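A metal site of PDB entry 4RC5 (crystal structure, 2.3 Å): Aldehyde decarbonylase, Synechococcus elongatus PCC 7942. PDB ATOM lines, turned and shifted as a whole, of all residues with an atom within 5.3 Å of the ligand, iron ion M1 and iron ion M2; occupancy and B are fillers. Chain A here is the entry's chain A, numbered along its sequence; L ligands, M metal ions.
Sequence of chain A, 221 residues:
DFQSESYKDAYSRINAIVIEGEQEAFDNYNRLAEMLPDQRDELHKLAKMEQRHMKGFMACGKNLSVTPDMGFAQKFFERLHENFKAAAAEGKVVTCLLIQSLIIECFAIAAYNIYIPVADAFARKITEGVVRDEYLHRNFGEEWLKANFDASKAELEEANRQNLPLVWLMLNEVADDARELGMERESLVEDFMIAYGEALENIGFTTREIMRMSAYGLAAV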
ATOM      1  N   TYR A  11      20.108 -24.600 -14.166  1.00  0.00           N
ATOM      2  CA  TYR A  11      19.618 -23.401 -13.514  1.00  0.00           C
ATOM      3  C   TYR A  11      19.847 -22.168 -14.389  1.00  0.00           C
ATOM      4  O   TYR A  11      19.022 -21.235 -14.415  1.00  0.00           O
ATOM      5  CB  TYR A  11      20.232 -23.198 -12.107  1.00  0.00           C
ATOM      6  CG  TYR A  11      19.282 -22.469 -11.213  1.00  0.00           C
ATOM      7  CD1 TYR A  11      18.267 -23.151 -10.517  1.00  0.00           C
ATOM      8  CD2 TYR A  11      19.321 -21.088 -11.097  1.00  0.00           C
ATOM      9  CE1 TYR A  11      17.377 -22.473  -9.712  1.00  0.00           C
ATOM     10  CE2 TYR A  11      18.418 -20.408 -10.286  1.00  0.00           C
ATOM     11  CZ  TYR A  11      17.457 -21.123  -9.595  1.00  0.00           C
ATOM     12  OH  TYR A  11      16.562 -20.416  -8.796  1.00  0.00           O
ATOM     13  N   ILE A  14      16.773 -22.304 -16.703  1.00  0.00           N
ATOM     14  CA  ILE A  14      15.505 -22.203 -15.984  1.00  0.00           C
ATOM     15  C   ILE A  14      15.353 -20.837 -15.354  1.00  0.00           C
ATOM     16  O   ILE A  14      14.306 -20.214 -15.458  1.00  0.00           O
ATOM     17  CB  ILE A  14      15.360 -23.261 -14.863  1.00  0.00           C
ATOM     18  CG1 ILE A  14      15.249 -24.652 -15.438  1.00  0.00           C
ATOM     19  CG2 ILE A  14      14.133 -22.955 -13.970  1.00  0.00           C
ATOM     20  CD1 ILE A  14      13.963 -24.960 -16.104  1.00  0.00           C
ATOM     21  N   ASN A  15      16.387 -20.377 -14.679  1.00  0.00           N
ATOM     22  CA  ASN A  15      16.398 -19.036 -14.112  1.00  0.00           C
ATOM     23  C   ASN A  15      16.171 -17.958 -15.172  1.00  0.00           C
ATOM     24  O   ASN A  15      15.412 -17.006 -14.962  1.00  0.00           O
ATOM     25  CB  ASN A  15      17.723 -18.798 -13.435  1.00  0.00           C
ATOM     26  CG  ASN A  15      17.777 -17.467 -12.722  1.00  0.00           C
ATOM     27  OD1 ASN A  15      18.733 -16.706 -12.914  1.00  0.00           O
ATOM     28  ND2 ASN A  15      16.783 -17.191 -11.893  1.00  0.00           N
ATOM     29  N   ILE A  17      14.694 -18.413 -18.127  1.00  0.00           N
ATOM     30  CA  ILE A  17      13.342 -18.573 -18.654  1.00  0.00           C
ATOM     31  C   ILE A  17      12.329 -17.915 -17.732  1.00  0.00           C
ATOM     32  O   ILE A  17      11.423 -17.199 -18.202  1.00  0.00           O
ATOM     33  CB  ILE A  17      12.972 -20.056 -18.831  1.00  0.00           C
ATOM     34  CG1 ILE A  17      13.524 -20.579 -20.168  1.00  0.00           C
ATOM     35  CG2 ILE A  17      11.471 -20.239 -18.768  1.00  0.00           C
ATOM     36  CD1 ILE A  17      13.552 -22.098 -20.257  1.00  0.00           C
ATOM     37  N   VAL A  18      12.478 -18.142 -16.435  1.00  0.00           N
ATOM     38  CA  VAL A  18      11.576 -17.566 -15.447  1.00  0.00           C
ATOM     39  C   VAL A  18      11.667 -16.046 -15.459  1.00  0.00           C
ATOM     40  O   VAL A  18      10.668 -15.351 -15.390  1.00  0.00           O
ATOM     41  CB  VAL A  18      11.879 -18.100 -14.034  1.00  0.00           C
ATOM     42  CG1 VAL A  18      11.637 -17.008 -13.009  1.00  0.00           C
ATOM     43  CG2 VAL A  18      11.022 -19.343 -13.737  1.00  0.00           C
ATOM     44  N   GLY A  21       9.874 -14.599 -18.404  1.00  0.00           N
ATOM     45  CA  GLY A  21       8.439 -14.655 -18.199  1.00  0.00           C
ATOM     46  C   GLY A  21       7.938 -13.502 -17.380  1.00  0.00           C
ATOM     47  O   GLY A  21       6.932 -12.882 -17.720  1.00  0.00           O
ATOM     48  N   GLU A  22       8.637 -13.209 -16.287  1.00  0.00           N
ATOM     49  CA  GLU A  22       8.266 -12.108 -15.405  1.00  0.00           C
ATOM     50  C   GLU A  22       8.419 -10.777 -16.128  1.00  0.00           C
ATOM     51  O   GLU A  22       7.551  -9.916 -16.047  1.00  0.00           O
ATOM     52  CB  GLU A  22       9.116 -12.130 -14.131  1.00  0.00           C
ATOM     53  CG  GLU A  22       8.830 -13.313 -13.212  1.00  0.00           C
ATOM     54  CD  GLU A  22       7.381 -13.417 -12.832  1.00  0.00           C
ATOM     55  OE1 GLU A  22       6.644 -12.416 -12.968  1.00  0.00           O
ATOM     56  OE2 GLU A  22       6.953 -14.510 -12.388  1.00  0.00           O
ATOM     57  N   ALA A  25       5.873 -10.574 -18.908  1.00  0.00           N
ATOM     58  CA  ALA A  25       4.557 -10.371 -18.300  1.00  0.00           C
ATOM     59  C   ALA A  25       4.337  -8.886 -17.982  1.00  0.00           C
ATOM     60  O   ALA A  25       3.227  -8.371 -18.127  1.00  0.00           O
ATOM     61  CB  ALA A  25       4.393 -11.209 -17.053  1.00  0.00           C
ATOM     62  N   TYR A  29       0.907  -6.954 -19.318  1.00  0.00           N
ATOM     63  CA  TYR A  29      -0.064  -6.233 -18.483  1.00  0.00           C
ATOM     64  C   TYR A  29      -0.132  -4.716 -18.752  1.00  0.00           C
ATOM     65  O   TYR A  29      -1.235  -4.174 -18.793  1.00  0.00           O
ATOM     66  CB  TYR A  29       0.077  -6.560 -17.011  1.00  0.00           C
ATOM     67  CG  TYR A  29      -0.389  -7.959 -16.712  1.00  0.00           C
ATOM     68  CD1 TYR A  29      -1.684  -8.366 -17.017  1.00  0.00           C
ATOM     69  CD2 TYR A  29       0.478  -8.870 -16.112  1.00  0.00           C
ATOM     70  CE1 TYR A  29      -2.104  -9.657 -16.733  1.00  0.00           C
ATOM     71  CE2 TYR A  29       0.071 -10.179 -15.826  1.00  0.00           C
ATOM     72  CZ  TYR A  29      -1.217 -10.559 -16.142  1.00  0.00           C
ATOM     73  OH  TYR A  29      -1.625 -11.831 -15.858  1.00  0.00           O
ATOM     74  N   GLU A  50       4.801  -7.940 -11.590  1.00  0.00           N
ATOM     75  CA  GLU A  50       5.729  -8.714 -12.427  1.00  0.00           C
ATOM     76  C   GLU A  50       7.189  -8.182 -12.360  1.00  0.00           C
ATOM     77  O   GLU A  50       8.152  -8.969 -12.336  1.00  0.00           O
ATOM     78  CB  GLU A  50       5.239  -8.799 -13.885  1.00  0.00           C
ATOM     79  CG  GLU A  50       3.801  -9.265 -14.049  1.00  0.00           C
ATOM     80  CD  GLU A  50       3.582 -10.740 -13.716  1.00  0.00           C
ATOM     81  OE1 GLU A  50       4.404 -11.378 -13.000  1.00  0.00           O
ATOM     82  OE2 GLU A  50       2.542 -11.300 -14.192  1.00  0.00           O
ATOM     83  N   HIS A  53       8.806  -9.538  -9.374  1.00  0.00           N
ATOM     84  CA  HIS A  53       9.148 -10.944  -9.548  1.00  0.00           C
ATOM     85  C   HIS A  53      10.415 -11.086 -10.303  1.00  0.00           C
ATOM     86  O   HIS A  53      11.230 -11.941  -9.956  1.00  0.00           O
ATOM     87  CB  HIS A  53       8.077 -11.706 -10.332  1.00  0.00           C
ATOM     88  CG  HIS A  53       6.720 -11.640  -9.703  1.00  0.00           C
ATOM     89  ND1 HIS A  53       5.632 -12.016 -10.358  1.00  0.00           N
ATOM     90  CD2 HIS A  53       6.310 -11.208  -8.449  1.00  0.00           C
ATOM     91  CE1 HIS A  53       4.546 -11.852  -9.562  1.00  0.00           C
ATOM     92  NE2 HIS A  53       4.971 -11.348  -8.395  1.00  0.00           N
ATOM     93  N   PHE A  57      13.761 -13.052  -9.067  1.00  0.00           N
ATOM     94  CA  PHE A  57      14.453 -14.163  -9.730  1.00  0.00           C
ATOM     95  C   PHE A  57      15.863 -13.854 -10.243  1.00  0.00           C
ATOM     96  O   PHE A  57      16.717 -14.732 -10.278  1.00  0.00           O
ATOM     97  CB  PHE A  57      13.583 -14.755 -10.848  1.00  0.00           C
ATOM     98  CG  PHE A  57      12.415 -15.533 -10.305  1.00  0.00           C
ATOM     99  CD1 PHE A  57      12.627 -16.629  -9.454  1.00  0.00           C
ATOM    100  CD2 PHE A  57      11.108 -15.145 -10.600  1.00  0.00           C
ATOM    101  CE1 PHE A  57      11.555 -17.325  -8.942  1.00  0.00           C
ATOM    102  CE2 PHE A  57      10.026 -15.866 -10.100  1.00  0.00           C
ATOM    103  CZ  PHE A  57      10.242 -16.959  -9.258  1.00  0.00           C
ATOM    104  N   PHE A  76      12.960 -19.357 -26.245  1.00  0.00           N
ATOM    105  CA  PHE A  76      11.893 -20.170 -25.556  1.00  0.00           C
ATOM    106  C   PHE A  76      10.530 -19.508 -25.659  1.00  0.00           C
ATOM    107  O   PHE A  76       9.529 -20.169 -25.994  1.00  0.00           O
ATOM    108  CB  PHE A  76      12.289 -20.331 -24.079  1.00  0.00           C
ATOM    109  CG  PHE A  76      11.378 -21.233 -23.255  1.00  0.00           C
ATOM    110  CD1 PHE A  76      11.482 -22.626 -23.349  1.00  0.00           C
ATOM    111  CD2 PHE A  76      10.483 -20.677 -22.327  1.00  0.00           C
ATOM    112  CE1 PHE A  76      10.685 -23.454 -22.550  1.00  0.00           C
ATOM    113  CE2 PHE A  76       9.670 -21.517 -21.539  1.00  0.00           C
ATOM    114  CZ  PHE A  76       9.791 -22.910 -21.648  1.00  0.00           C
ATOM    115  N   PHE A  77      10.504 -18.203 -25.412  1.00  0.00           N
ATOM    116  CA  PHE A  77       9.276 -17.423 -25.341  1.00  0.00           C
ATOM    117  C   PHE A  77       8.800 -16.796 -26.651  1.00  0.00           C
ATOM    118  O   PHE A  77       7.658 -16.344 -26.739  1.00  0.00           O
ATOM    119  CB  PHE A  77       9.453 -16.280 -24.319  1.00  0.00           C
ATOM    120  CG  PHE A  77       9.040 -16.655 -22.946  1.00  0.00           C
ATOM    121  CD1 PHE A  77       7.669 -16.728 -22.598  1.00  0.00           C
ATOM    122  CD2 PHE A  77       9.985 -16.954 -21.984  1.00  0.00           C
ATOM    123  CE1 PHE A  77       7.289 -17.086 -21.330  1.00  0.00           C
ATOM    124  CE2 PHE A  77       9.596 -17.318 -20.700  1.00  0.00           C
ATOM    125  CZ  PHE A  77       8.255 -17.377 -20.379  1.00  0.00           C
ATOM    126  N   GLN A 100      -1.692 -14.382 -21.526  1.00  0.00           N
ATOM    127  CA  GLN A 100      -1.039 -13.989 -20.334  1.00  0.00           C
ATOM    128  C   GLN A 100      -1.714 -14.358 -19.034  1.00  0.00           C
ATOM    129  O   GLN A 100      -1.139 -14.983 -18.207  1.00  0.00           O
ATOM    130  CB  GLN A 100      -0.675 -12.507 -20.358  1.00  0.00           C
ATOM    131  CG  GLN A 100      -0.040 -12.056 -19.076  1.00  0.00           C
ATOM    132  CD  GLN A 100       1.317 -12.656 -18.807  1.00  0.00           C
ATOM    133  OE1 GLN A 100       2.102 -12.791 -19.666  1.00  0.00           O
ATOM    134  NE2 GLN A 100       1.592 -12.955 -17.618  1.00  0.00           N
ATOM    135  N   ILE A 104      -0.531 -18.644 -19.648  1.00  0.00           N
ATOM    136  CA  ILE A 104       0.753 -18.339 -19.019  1.00  0.00           C
ATOM    137  C   ILE A 104       0.808 -18.285 -17.512  1.00  0.00           C
ATOM    138  O   ILE A 104       1.644 -18.885 -16.951  1.00  0.00           O
ATOM    139  CB  ILE A 104       1.424 -17.063 -19.575  1.00  0.00           C
ATOM    140  CG1 ILE A 104       1.997 -17.317 -20.961  1.00  0.00           C
ATOM    141  CG2 ILE A 104       2.564 -16.505 -18.712  1.00  0.00           C
ATOM    142  CD1 ILE A 104       2.631 -16.087 -21.561  1.00  0.00           C
ATOM    143  N   GLU A 105       0.009 -17.433 -16.888  1.00  0.00           N
ATOM    144  CA  GLU A 105      -0.079 -17.424 -15.432  1.00  0.00           C
ATOM    145  C   GLU A 105      -0.153 -18.855 -14.909  1.00  0.00           C
ATOM    146  O   GLU A 105       0.686 -19.284 -14.121  1.00  0.00           O
ATOM    147  CB  GLU A 105      -1.312 -16.635 -15.002  1.00  0.00           C
ATOM    148  CG  GLU A 105      -1.165 -15.133 -15.142  1.00  0.00           C
ATOM    149  CD  GLU A 105      -0.057 -14.570 -14.282  1.00  0.00           C
ATOM    150  OE1 GLU A 105       0.075 -15.006 -13.126  1.00  0.00           O
ATOM    151  OE2 GLU A 105       0.692 -13.691 -14.766  1.00  0.00           O
ATOM    152  N   PHE A 107       0.634 -21.616 -16.141  1.00  0.00           N
ATOM    153  CA  PHE A 107       1.891 -22.324 -16.350  1.00  0.00           C
ATOM    154  C   PHE A 107       2.890 -22.020 -15.228  1.00  0.00           C
ATOM    155  O   PHE A 107       3.578 -22.912 -14.748  1.00  0.00           O
ATOM    156  CB  PHE A 107       2.495 -21.944 -17.706  1.00  0.00           C
ATOM    157  CG  PHE A 107       3.686 -22.776 -18.089  1.00  0.00           C
ATOM    158  CD1 PHE A 107       3.701 -24.141 -17.860  1.00  0.00           C
ATOM    159  CD2 PHE A 107       4.802 -22.185 -18.668  1.00  0.00           C
ATOM    160  CE1 PHE A 107       4.799 -24.911 -18.215  1.00  0.00           C
ATOM    161  CE2 PHE A 107       5.904 -22.947 -19.019  1.00  0.00           C
ATOM    162  CZ  PHE A 107       5.898 -24.305 -18.787  1.00  0.00           C
ATOM    163  N   ALA A 108       2.957 -20.760 -14.831  1.00  0.00           N
ATOM    164  CA  ALA A 108       3.869 -20.335 -13.776  1.00  0.00           C
ATOM    165  C   ALA A 108       3.426 -20.869 -12.418  1.00  0.00           C
ATOM    166  O   ALA A 108       4.252 -21.155 -11.549  1.00  0.00           O
ATOM    167  CB  ALA A 108       3.980 -18.820 -13.745  1.00  0.00           C
ATOM    168  N   ALA A 111       4.336 -24.755 -12.251  1.00  0.00           N
ATOM    169  CA  ALA A 111       5.787 -24.964 -12.213  1.00  0.00           C
ATOM    170  C   ALA A 111       6.392 -24.385 -10.943  1.00  0.00           C
ATOM    171  O   ALA A 111       7.204 -25.023 -10.266  1.00  0.00           O
ATOM    172  CB  ALA A 111       6.435 -24.328 -13.423  1.00  0.00           C
ATOM    173  N   TYR A 112       6.014 -23.161 -10.620  1.00  0.00           N
ATOM    174  CA  TYR A 112       6.457 -22.553  -9.390  1.00  0.00           C
ATOM    175  C   TYR A 112       6.113 -23.376  -8.161  1.00  0.00           C
ATOM    176  O   TYR A 112       6.974 -23.578  -7.318  1.00  0.00           O
ATOM    177  CB  TYR A 112       5.957 -21.120  -9.276  1.00  0.00           C
ATOM    178  CG  TYR A 112       6.597 -20.203 -10.280  1.00  0.00           C
ATOM    179  CD1 TYR A 112       7.337 -20.691 -11.348  1.00  0.00           C
ATOM    180  CD2 TYR A 112       6.420 -18.844 -10.175  1.00  0.00           C
ATOM    181  CE1 TYR A 112       7.911 -19.844 -12.278  1.00  0.00           C
ATOM    182  CE2 TYR A 112       7.010 -17.969 -11.101  1.00  0.00           C
ATOM    183  CZ  TYR A 112       7.749 -18.483 -12.142  1.00  0.00           C
ATOM    184  OH  TYR A 112       8.298 -17.621 -13.081  1.00  0.00           O
ATOM    185  N   TYR A 115       8.409 -26.211  -8.078  1.00  0.00           N
ATOM    186  CA  TYR A 115       9.744 -25.818  -7.734  1.00  0.00           C
ATOM    187  C   TYR A 115       9.950 -25.584  -6.212  1.00  0.00           C
ATOM    188  O   TYR A 115      11.002 -25.933  -5.664  1.00  0.00           O
ATOM    189  CB  TYR A 115      10.172 -24.611  -8.562  1.00  0.00           C
ATOM    190  CG  TYR A 115      11.509 -24.010  -8.178  1.00  0.00           C
ATOM    191  CD1 TYR A 115      12.705 -24.750  -8.299  1.00  0.00           C
ATOM    192  CD2 TYR A 115      11.596 -22.689  -7.729  1.00  0.00           C
ATOM    193  CE1 TYR A 115      13.922 -24.181  -7.940  1.00  0.00           C
ATOM    194  CE2 TYR A 115      12.806 -22.126  -7.398  1.00  0.00           C
ATOM    195  CZ  TYR A 115      13.953 -22.878  -7.502  1.00  0.00           C
ATOM    196  OH  TYR A 115      15.153 -22.300  -7.148  1.00  0.00           O
ATOM    197  N   THR A 127      10.162 -17.442  -4.288  1.00  0.00           N
ATOM    198  CA  THR A 127       9.124 -18.077  -5.087  1.00  0.00           C
ATOM    199  C   THR A 127       7.743 -18.128  -4.377  1.00  0.00           C
ATOM    200  O   THR A 127       6.728 -17.900  -5.001  1.00  0.00           O
ATOM    201  CB  THR A 127       9.574 -19.492  -5.568  1.00  0.00           C
ATOM    202  OG1 THR A 127      10.868 -19.373  -6.221  1.00  0.00           O
ATOM    203  CG2 THR A 127       8.565 -20.134  -6.540  1.00  0.00           C
ATOM    204  N   GLU A 134       0.605 -14.584  -8.434  1.00  0.00           N
ATOM    205  CA  GLU A 134       0.089 -15.247  -9.614  1.00  0.00           C
ATOM    206  C   GLU A 134      -1.357 -15.645  -9.483  1.00  0.00           C
ATOM    207  O   GLU A 134      -2.092 -15.571 -10.462  1.00  0.00           O
ATOM    208  CB  GLU A 134       0.977 -16.465 -10.000  1.00  0.00           C
ATOM    209  CG  GLU A 134       2.426 -16.027 -10.141  1.00  0.00           C
ATOM    210  CD  GLU A 134       3.341 -17.052 -10.735  1.00  0.00           C
ATOM    211  OE1 GLU A 134       3.222 -18.264 -10.413  1.00  0.00           O
ATOM    212  OE2 GLU A 134       4.235 -16.600 -11.515  1.00  0.00           O
ATOM    213  N   HIS A 137      -3.323 -12.667 -10.562  1.00  0.00           N
ATOM    214  CA  HIS A 137      -3.296 -12.400 -11.990  1.00  0.00           C
ATOM    215  C   HIS A 137      -4.240 -13.295 -12.737  1.00  0.00           C
ATOM    216  O   HIS A 137      -4.989 -12.821 -13.570  1.00  0.00           O
ATOM    217  CB  HIS A 137      -1.878 -12.642 -12.536  1.00  0.00           C
ATOM    218  CG  HIS A 137      -0.833 -11.782 -11.898  1.00  0.00           C
ATOM    219  ND1 HIS A 137       0.441 -11.797 -12.299  1.00  0.00           N
ATOM    220  CD2 HIS A 137      -0.927 -10.810 -10.879  1.00  0.00           C
ATOM    221  CE1 HIS A 137       1.136 -10.893 -11.548  1.00  0.00           C
ATOM    222  NE2 HIS A 137       0.305 -10.313 -10.696  1.00  0.00           N
ATOM    223  N   VAL A 174      11.451 -27.434 -21.497  1.00  0.00           N
ATOM    224  CA  VAL A 174      12.063 -27.298 -20.169  1.00  0.00           C
ATOM    225  C   VAL A 174      12.221 -28.633 -19.441  1.00  0.00           C
ATOM    226  O   VAL A 174      12.904 -28.686 -18.412  1.00  0.00           O
ATOM    227  CB  VAL A 174      11.302 -26.369 -19.190  1.00  0.00           C
ATOM    228  CG1 VAL A 174      11.483 -24.928 -19.540  1.00  0.00           C
ATOM    229  CG2 VAL A 174       9.849 -26.727 -19.038  1.00  0.00           C
ATOM    230  N   LEU A 181      16.627 -29.984 -11.689  1.00  0.00           N
ATOM    231  CA  LEU A 181      16.263 -29.162 -10.527  1.00  0.00           C
ATOM    232  C   LEU A 181      15.324 -29.869  -9.520  1.00  0.00           C
ATOM    233  O   LEU A 181      14.926 -29.283  -8.504  1.00  0.00           O
ATOM    234  CB  LEU A 181      15.620 -27.854 -11.011  1.00  0.00           C
ATOM    235  CG  LEU A 181      16.499 -26.634 -11.234  1.00  0.00           C
ATOM    236  CD1 LEU A 181      17.528 -26.916 -12.291  1.00  0.00           C
ATOM    237  CD2 LEU A 181      15.675 -25.415 -11.628  1.00  0.00           C
ATOM    238  N   MET A 183      12.276 -31.384 -10.421  1.00  0.00           N
ATOM    239  CA  MET A 183      10.894 -31.155 -10.812  1.00  0.00           C
ATOM    240  C   MET A 183      10.465 -32.177 -11.881  1.00  0.00           C
ATOM    241  O   MET A 183      10.968 -32.133 -12.993  1.00  0.00           O
ATOM    242  CB  MET A 183      10.729 -29.737 -11.369  1.00  0.00           C
ATOM    243  CG  MET A 183      11.217 -28.619 -10.486  1.00  0.00           C
ATOM    244  SD  MET A 183      10.898 -26.968 -11.180  1.00  0.00           S
ATOM    245  CE  MET A 183      12.164 -26.772 -12.380  1.00  0.00           C
HETATM  246  C1  LIG L   1       4.639 -14.488 -14.988  1.00  0.00           C
HETATM  247  O1  LIG L   1       3.474 -14.116 -14.786  1.00  0.00           O
HETATM  248  C2  LIG L   1       4.943 -15.461 -16.133  1.00  0.00           C
HETATM  249  C3  LIG L   1       6.134 -16.374 -15.891  1.00  0.00           C
HETATM  250  C4  LIG L   1       6.007 -17.708 -16.607  1.00  0.00           C
HETATM  251  C5  LIG L   1       7.346 -18.435 -16.733  1.00  0.00           C
HETATM  252  C6  LIG L   1       7.068 -19.953 -16.850  1.00  0.00           C
HETATM  253  C7  LIG L   1       8.378 -20.771 -16.798  1.00  0.00           C
HETATM  254  C8  LIG L   1       8.069 -22.213 -16.501  1.00  0.00           C
HETATM  255  C9  LIG L   1       9.307 -23.062 -16.727  1.00  0.00           C
HETATM  256  C10 LIG L   1       9.843 -23.803 -15.478  1.00  0.00           C
HETATM  257  C11 LIG L   1       9.461 -23.143 -14.153  1.00  0.00           C
HETATM  258  C12 LIG L   1      10.640 -22.712 -13.308  1.00  0.00           C
HETATM  259  C13 LIG L   1      10.377 -22.665 -11.803  1.00  0.00           C
HETATM  260  C14 LIG L   1      11.663 -22.393 -11.020  1.00  0.00           C
HETATM  261  C15 LIG L   1      12.029 -20.917 -10.917  1.00  0.00           C
HETATM  262  C16 LIG L   1      13.511 -20.664 -10.540  1.00  0.00           C
HETATM  263 FE    FE M   1       2.025 -13.101 -13.330  1.00  0.00          FE
HETATM  264 FE    FE M   2       4.916 -13.160 -12.282  1.00  0.00          FE
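OH of Tyr 29 sits close to OE2 of Glu 105, 3.2 Å away. The side-chain hydroxyl of Tyr 112 lies close to the side-chain carboxylate of Glu 22, at 3.5 Å. OH of Tyr 115 lies within hydrogen-bond range of OH of Tyr 11, at 2.9 Å. N of Glu 105 sits at hydrogen-bond distance from O of Gln 100 (3.0 Å).
Residues that only touch the ligand: Tyr 115 (3.3 Å), Ala 111 (3.3 Å), Val 18 (3.4 Å), Phe 107 (3.4 Å), Tyr 11 (3.5 Å), Ile 14 (3.6 Å), Gln 100 (3.6 Å), Gly 21 (3.6 Å), Tyr 112 (3.7 Å), Ile 104 (3.7 Å), Ala 108 (3.7 Å), Ile 17 (3.7 Å), Ala 25 (3.8 Å) and Phe 77 (3.9 Å). Hydrophobic or aromatic side chains within 4 Å of the ligand: Ile 14, Ile 17, Val 18, Ala 25, Phe 77, Ile 104, Phe 107, Ala 108, Ala 111, Tyr 112 and Tyr 115. Within 4 Å of the ligand: Tyr 11, Ile 14, Ile 17, Val 18, Gly 21, Glu 22, Ala 25, Glu 50, Phe 77, Gln 100, Ile 104, Glu 105, Phe 107, Ala 108, Ala 111, Tyr 112 and Tyr 115.
Three residues have an atom within 4 Å of iron ion M1: Glu 50, Glu 105 and His 137.
Residues that only touch iron ion M2: Glu 134 (3.6 Å). Of the 28 residues printed, 4 come within 4 Å of iron ion M2.
Iron ion M1 is bound by OE2 of Glu 105 (2.0 Å), OE2 of Glu 50 (2.1 Å), O1 of the ligand (2.3 Å) and ND1 of His 137 (2.3 Å). Iron ion M1 has four donor atoms within binding distance. Slightly farther from iron ion M1 lies the side-chain carboxylate (OE1) of Glu 105 (2.7 Å).
Iron ion M2 is bound by the side-chain carboxylate (OE1) of Glu 50, the side-chain carboxylate (OE1) of Glu 22, a ring nitrogen (ND1) of His 53 and the side-chain carboxylate (OE2) of Glu 22. Iron ion M2 has four donor atoms within binding distance.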
